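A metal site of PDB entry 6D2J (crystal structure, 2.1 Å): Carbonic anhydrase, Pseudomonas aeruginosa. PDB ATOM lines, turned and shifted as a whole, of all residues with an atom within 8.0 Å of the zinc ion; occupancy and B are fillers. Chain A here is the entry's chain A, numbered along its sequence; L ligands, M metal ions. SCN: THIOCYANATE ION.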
ATOM      1  N   GLY A  39     -13.891  15.619 -10.076  1.00  0.00           N
ATOM      2  CA  GLY A  39     -13.063  16.816 -10.094  1.00  0.00           C
ATOM      3  C   GLY A  39     -11.632  16.583  -9.687  1.00  0.00           C
ATOM      4  O   GLY A  39     -11.189  15.444  -9.488  1.00  0.00           O
ATOM      5  N   CYS A  40     -10.891  17.686  -9.557  1.00  0.00           N
ATOM      6  CA  CYS A  40      -9.492  17.614  -9.169  1.00  0.00           C
ATOM      7  C   CYS A  40      -9.327  17.492  -7.669  1.00  0.00           C
ATOM      8  O   CYS A  40     -10.158  18.001  -6.894  1.00  0.00           O
ATOM      9  CB  CYS A  40      -8.726  18.847  -9.661  1.00  0.00           C
ATOM     10  SG  CYS A  40      -6.930  18.712  -9.363  1.00  0.00           S
ATOM     11  N   SER A  41      -8.239  16.830  -7.253  1.00  0.00           N
ATOM     12  CA  SER A  41      -7.840  16.696  -5.859  1.00  0.00           C
ATOM     13  C   SER A  41      -7.457  18.039  -5.209  1.00  0.00           C
ATOM     14  O   SER A  41      -7.447  18.123  -3.983  1.00  0.00           O
ATOM     15  CB  SER A  41      -6.643  15.731  -5.750  1.00  0.00           C
ATOM     16  OG  SER A  41      -7.039  14.406  -6.117  1.00  0.00           O
ATOM     17  N   ASP A  42      -7.123  19.037  -6.028  1.00  0.00           N
ATOM     18  CA  ASP A  42      -6.698  20.370  -5.572  1.00  0.00           C
ATOM     19  C   ASP A  42      -7.558  20.833  -4.386  1.00  0.00           C
ATOM     20  O   ASP A  42      -8.785  20.880  -4.483  1.00  0.00           O
ATOM     21  CB  ASP A  42      -6.765  21.382  -6.728  1.00  0.00           C
ATOM     22  CG  ASP A  42      -6.175  22.755  -6.374  1.00  0.00           C
ATOM     23  OD1 ASP A  42      -5.283  23.225  -7.121  1.00  0.00           O
ATOM     24  OD2 ASP A  42      -6.621  23.381  -5.378  1.00  0.00           O
ATOM     25  N   ALA A  43      -6.900  21.175  -3.283  1.00  0.00           N
ATOM     26  CA  ALA A  43      -7.567  21.541  -2.030  1.00  0.00           C
ATOM     27  C   ALA A  43      -8.512  22.736  -2.161  1.00  0.00           C
ATOM     28  O   ALA A  43      -9.400  22.928  -1.326  1.00  0.00           O
ATOM     29  CB  ALA A  43      -6.547  21.830  -0.947  1.00  0.00           C
ATOM     30  N   ARG A  44      -8.310  23.551  -3.201  1.00  0.00           N
ATOM     31  CA  ARG A  44      -9.095  24.755  -3.360  1.00  0.00           C
ATOM     32  C   ARG A  44     -10.371  24.506  -4.168  1.00  0.00           C
ATOM     33  O   ARG A  44     -11.122  25.436  -4.473  1.00  0.00           O
ATOM     34  CB  ARG A  44      -8.228  25.846  -4.008  1.00  0.00           C
ATOM     35  CG  ARG A  44      -6.976  26.161  -3.177  1.00  0.00           C
ATOM     36  CD  ARG A  44      -5.917  26.880  -3.988  1.00  0.00           C
ATOM     37  NE  ARG A  44      -5.449  26.067  -5.106  1.00  0.00           N
ATOM     38  CZ  ARG A  44      -4.514  26.451  -5.964  1.00  0.00           C
ATOM     39  NH1 ARG A  44      -3.944  27.638  -5.828  1.00  0.00           N
ATOM     40  NH2 ARG A  44      -4.157  25.645  -6.961  1.00  0.00           N
ATOM     41  N   VAL A  45     -10.646  23.248  -4.505  1.00  0.00           N
ATOM     42  CA  VAL A  45     -11.858  22.966  -5.290  1.00  0.00           C
ATOM     43  C   VAL A  45     -12.755  21.926  -4.605  1.00  0.00           C
ATOM     44  O   VAL A  45     -13.063  20.882  -5.182  1.00  0.00           O
ATOM     45  CB  VAL A  45     -11.491  22.523  -6.729  1.00  0.00           C
ATOM     46  CG1 VAL A  45     -12.692  22.649  -7.680  1.00  0.00           C
ATOM     47  CG2 VAL A  45     -10.338  23.388  -7.283  1.00  0.00           C
ATOM     48  N   ASN A  63      -9.281  13.213  -8.339  1.00  0.00           N
ATOM     49  CA  ASN A  63      -7.946  12.742  -8.648  1.00  0.00           C
ATOM     50  C   ASN A  63      -7.174  13.898  -9.257  1.00  0.00           C
ATOM     51  O   ASN A  63      -7.757  14.955  -9.518  1.00  0.00           O
ATOM     52  CB  ASN A  63      -7.989  11.510  -9.594  1.00  0.00           C
ATOM     53  CG  ASN A  63      -8.510  11.838 -11.014  1.00  0.00           C
ATOM     54  OD1 ASN A  63      -7.980  12.705 -11.717  1.00  0.00           O
ATOM     55  ND2 ASN A  63      -9.513  11.078 -11.450  1.00  0.00           N
ATOM     56  N   VAL A  64      -5.875  13.741  -9.475  1.00  0.00           N
ATOM     57  CA  VAL A  64      -5.103  14.889  -9.942  1.00  0.00           C
ATOM     58  C   VAL A  64      -5.441  15.226 -11.390  1.00  0.00           C
ATOM     59  O   VAL A  64      -5.243  14.413 -12.322  1.00  0.00           O
ATOM     60  CB  VAL A  64      -3.579  14.678  -9.806  1.00  0.00           C
ATOM     61  CG1 VAL A  64      -2.849  15.879 -10.417  1.00  0.00           C
ATOM     62  CG2 VAL A  64      -3.192  14.531  -8.348  1.00  0.00           C
ATOM     63  N   ALA A  65      -5.979  16.431 -11.550  1.00  0.00           N
ATOM     64  CA  ALA A  65      -6.425  17.013 -12.818  1.00  0.00           C
ATOM     65  C   ALA A  65      -7.641  16.299 -13.419  1.00  0.00           C
ATOM     66  O   ALA A  65      -7.823  16.297 -14.638  1.00  0.00           O
ATOM     67  CB  ALA A  65      -5.258  17.064 -13.840  1.00  0.00           C
ATOM     68  N   ASN A  66      -8.491  15.746 -12.563  1.00  0.00           N
ATOM     69  CA  ASN A  66      -9.831  15.227 -12.969  1.00  0.00           C
ATOM     70  C   ASN A  66      -9.844  14.428 -14.284  1.00  0.00           C
ATOM     71  O   ASN A  66     -10.615  14.695 -15.231  1.00  0.00           O
ATOM     72  CB  ASN A  66     -10.856  16.385 -13.024  1.00  0.00           C
ATOM     73  CG  ASN A  66     -10.370  17.591 -13.827  1.00  0.00           C
ATOM     74  OD1 ASN A  66      -9.774  18.518 -13.262  1.00  0.00           O
ATOM     75  ND2 ASN A  66     -10.690  17.614 -15.119  1.00  0.00           N
ATOM     76  N   THR A  94     -15.799  18.495 -13.517  1.00  0.00           N
ATOM     77  CA  THR A  94     -15.361  19.844 -13.185  1.00  0.00           C
ATOM     78  C   THR A  94     -13.846  19.931 -13.082  1.00  0.00           C
ATOM     79  O   THR A  94     -13.235  19.320 -12.199  1.00  0.00           O
ATOM     80  CB  THR A  94     -15.965  20.322 -11.842  1.00  0.00           C
ATOM     81  OG1 THR A  94     -17.398  20.265 -11.916  1.00  0.00           O
ATOM     82  CG2 THR A  94     -15.534  21.774 -11.523  1.00  0.00           C
ATOM     83  N   GLY A  95     -13.236  20.669 -14.015  1.00  0.00           N
ATOM     84  CA  GLY A  95     -11.817  20.957 -13.925  1.00  0.00           C
ATOM     85  C   GLY A  95     -11.714  22.342 -13.303  1.00  0.00           C
ATOM     86  O   GLY A  95     -12.739  22.915 -12.890  1.00  0.00           O
ATOM     87  N   HIS A  96     -10.502  22.875 -13.211  1.00  0.00           N
ATOM     88  CA  HIS A  96     -10.362  24.236 -12.695  1.00  0.00           C
ATOM     89  C   HIS A  96      -9.200  24.940 -13.362  1.00  0.00           C
ATOM     90  O   HIS A  96      -8.241  24.299 -13.796  1.00  0.00           O
ATOM     91  CB  HIS A  96     -10.190  24.232 -11.160  1.00  0.00           C
ATOM     92  CG  HIS A  96      -8.938  23.556 -10.701  1.00  0.00           C
ATOM     93  ND1 HIS A  96      -7.807  24.253 -10.354  1.00  0.00           N
ATOM     94  CD2 HIS A  96      -8.635  22.247 -10.542  1.00  0.00           C
ATOM     95  CE1 HIS A  96      -6.859  23.408  -9.998  1.00  0.00           C
ATOM     96  NE2 HIS A  96      -7.342  22.184 -10.105  1.00  0.00           N
ATOM     97  N   TYR A  97      -9.309  26.258 -13.465  1.00  0.00           N
ATOM     98  CA  TYR A  97      -8.239  27.077 -14.009  1.00  0.00           C
ATOM     99  C   TYR A  97      -7.023  27.030 -13.077  1.00  0.00           C
ATOM    100  O   TYR A  97      -7.170  26.795 -11.873  1.00  0.00           O
ATOM    101  CB  TYR A  97      -8.704  28.513 -14.192  1.00  0.00           C
ATOM    102  CG  TYR A  97      -9.727  28.669 -15.278  1.00  0.00           C
ATOM    103  CD1 TYR A  97     -11.013  29.098 -15.002  1.00  0.00           C
ATOM    104  CD2 TYR A  97      -9.404  28.365 -16.604  1.00  0.00           C
ATOM    105  CE1 TYR A  97     -11.956  29.226 -16.001  1.00  0.00           C
ATOM    106  CE2 TYR A  97     -10.330  28.489 -17.620  1.00  0.00           C
ATOM    107  CZ  TYR A  97     -11.611  28.935 -17.307  1.00  0.00           C
ATOM    108  OH  TYR A  97     -12.546  29.073 -18.312  1.00  0.00           O
ATOM    109  N   GLY A  98      -5.831  27.226 -13.653  1.00  0.00           N
ATOM    110  CA  GLY A  98      -4.593  27.156 -12.898  1.00  0.00           C
ATOM    111  C   GLY A  98      -4.234  25.775 -12.351  1.00  0.00           C
ATOM    112  O   GLY A  98      -3.458  25.656 -11.410  1.00  0.00           O
ATOM    113  N   CYS A  99      -4.788  24.719 -12.949  1.00  0.00           N
ATOM    114  CA  CYS A  99      -4.591  23.370 -12.432  1.00  0.00           C
ATOM    115  C   CYS A  99      -3.112  22.965 -12.541  1.00  0.00           C
ATOM    116  O   CYS A  99      -2.517  23.050 -13.618  1.00  0.00           O
ATOM    117  CB  CYS A  99      -5.492  22.373 -13.176  1.00  0.00           C
ATOM    118  SG  CYS A  99      -5.317  20.625 -12.683  1.00  0.00           S
ATOM    119  N   GLY A 100      -2.515  22.556 -11.416  1.00  0.00           N
ATOM    120  CA  GLY A 100      -1.124  22.129 -11.401  1.00  0.00           C
ATOM    121  C   GLY A 100      -0.874  20.901 -12.275  1.00  0.00           C
ATOM    122  O   GLY A 100       0.176  20.795 -12.922  1.00  0.00           O
ATOM    123  N   GLY A 101      -1.822  19.975 -12.291  1.00  0.00           N
ATOM    124  CA  GLY A 101      -1.664  18.776 -13.114  1.00  0.00           C
ATOM    125  C   GLY A 101      -1.570  19.158 -14.579  1.00  0.00           C
ATOM    126  O   GLY A 101      -0.699  18.718 -15.319  1.00  0.00           O
ATOM    127  N   VAL A 102      -2.493  20.012 -15.002  1.00  0.00           N
ATOM    128  CA  VAL A 102      -2.511  20.519 -16.373  1.00  0.00           C
ATOM    129  C   VAL A 102      -1.230  21.296 -16.664  1.00  0.00           C
ATOM    130  O   VAL A 102      -0.613  21.109 -17.714  1.00  0.00           O
ATOM    131  CB  VAL A 102      -3.751  21.402 -16.612  1.00  0.00           C
ATOM    132  CG1 VAL A 102      -3.678  22.090 -17.944  1.00  0.00           C
ATOM    133  CG2 VAL A 102      -5.022  20.545 -16.488  1.00  0.00           C
ATOM    134  N   ARG A 103      -0.819  22.149 -15.725  1.00  0.00           N
ATOM    135  CA  ARG A 103       0.370  22.981 -15.923  1.00  0.00           C
ATOM    136  C   ARG A 103       1.630  22.134 -16.089  1.00  0.00           C
ATOM    137  O   ARG A 103       2.451  22.427 -16.957  1.00  0.00           O
ATOM    138  CB  ARG A 103       0.570  23.950 -14.755  1.00  0.00           C
ATOM    139  CG  ARG A 103       1.881  24.727 -14.851  1.00  0.00           C
ATOM    140  CD  ARG A 103       1.960  25.857 -13.832  1.00  0.00           C
ATOM    141  NE  ARG A 103       1.095  26.973 -14.184  1.00  0.00           N
ATOM    142  CZ  ARG A 103      -0.044  27.266 -13.546  1.00  0.00           C
ATOM    143  NH1 ARG A 103      -0.445  26.515 -12.535  1.00  0.00           N
ATOM    144  NH2 ARG A 103      -0.770  28.312 -13.930  1.00  0.00           N
ATOM    145  N   LEU A 118      -0.607  11.913 -15.907  1.00  0.00           N
ATOM    146  CA  LEU A 118      -0.960  13.126 -16.635  1.00  0.00           C
ATOM    147  C   LEU A 118      -0.695  13.056 -18.136  1.00  0.00           C
ATOM    148  O   LEU A 118      -0.978  14.003 -18.860  1.00  0.00           O
ATOM    149  CB  LEU A 118      -0.160  14.319 -16.052  1.00  0.00           C
ATOM    150  CG  LEU A 118      -0.415  14.641 -14.582  1.00  0.00           C
ATOM    151  CD1 LEU A 118       0.571  15.721 -14.140  1.00  0.00           C
ATOM    152  CD2 LEU A 118      -1.868  15.100 -14.448  1.00  0.00           C
ATOM    153  N   CYS A 146      -6.801  23.573 -19.594  1.00  0.00           N
ATOM    154  CA  CYS A 146      -7.719  23.150 -18.519  1.00  0.00           C
ATOM    155  C   CYS A 146      -9.107  22.911 -19.080  1.00  0.00           C
ATOM    156  O   CYS A 146      -9.764  21.914 -18.757  1.00  0.00           O
ATOM    157  CB  CYS A 146      -7.768  24.183 -17.402  1.00  0.00           C
ATOM    158  SG  CYS A 146      -6.277  24.228 -16.383  1.00  0.00           S
ATOM    159  N   ASN A 149      -9.169  19.922 -21.444  1.00  0.00           N
ATOM    160  CA  ASN A 149      -9.092  18.687 -20.692  1.00  0.00           C
ATOM    161  C   ASN A 149     -10.469  18.266 -20.192  1.00  0.00           C
ATOM    162  O   ASN A 149     -10.876  17.109 -20.402  1.00  0.00           O
ATOM    163  CB  ASN A 149      -8.113  18.817 -19.524  1.00  0.00           C
ATOM    164  CG  ASN A 149      -7.967  17.518 -18.760  1.00  0.00           C
ATOM    165  OD1 ASN A 149      -7.810  16.451 -19.366  1.00  0.00           O
ATOM    166  ND2 ASN A 149      -8.033  17.588 -17.430  1.00  0.00           N
ATOM    167  N   ILE A 182     -10.461  29.292  -9.481  1.00  0.00           N
ATOM    168  CA  ILE A 182      -9.906  29.416  -8.133  1.00  0.00           C
ATOM    169  C   ILE A 182      -9.697  30.887  -7.764  1.00  0.00           C
ATOM    170  O   ILE A 182      -9.664  31.237  -6.596  1.00  0.00           O
ATOM    171  CB  ILE A 182      -8.551  28.652  -7.976  1.00  0.00           C
ATOM    172  CG1 ILE A 182      -7.611  28.936  -9.164  1.00  0.00           C
ATOM    173  CG2 ILE A 182      -8.787  27.129  -7.793  1.00  0.00           C
ATOM    174  CD1 ILE A 182      -6.168  28.431  -8.962  1.00  0.00           C
HETATM  175  S   SCN L   1      -2.028  19.775  -8.224  1.00  0.00           S
HETATM  176  C   SCN L   1      -3.541  20.400  -8.889  1.00  0.00           C
HETATM  177  N   SCN L   1      -4.498  20.817  -9.314  1.00  0.00           N
HETATM  178 ZN    ZN M   1      -6.045  20.575 -10.434  1.00  0.00          ZN
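The zinc ion is bound by N of the ligand, at 1.9 Å.
The zinc ion is bound by NE2 of His 96.
SG of Cys 40 binds the zinc ion, at 2.3 Å.
SG of Cys 99 binds the zinc ion, 2.4 Å away.
The zinc ion has four donor atoms within binding distance.
The backbone carbonyl oxygen (O) of His 96 sits at hydrogen-bond distance from the side-chain sulfur (SG) of Cys 146 (3.2 Å).
The side-chain sulfur (SG) of Cys 40 sits close to the backbone NH (N) of Asp 42 (3.4 Å).
The side-chain sulfur of Cys 40 sits close to the backbone NH of Ala 65.
The side-chain sulfur of Cys 99 sits close to the backbone NH of Gly 101 (3.6 Å).
The side-chain sulfur (SG) of Cys 99 lies close to the backbone NH (N) of Val 102 (3.7 Å).
The backbone NH (N) of Cys 99 is in hydrogen-bond range of the side-chain sulfur (SG) of Cys 146, at 3.8 Å.
The guanidinium group (NH2) of Arg 44 lies within salt-bridge range of the side-chain carboxylate (OD1) of Asp 42 (2.7 Å).
Residues that only touch the zinc ion: Asp 42 (3.9 Å).
Of the 25 residues printed, 4 come within 4 Å of the zinc ion.
The nearest printed residue that does not touch the zinc ion is Gly 100 (4.2 Å).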
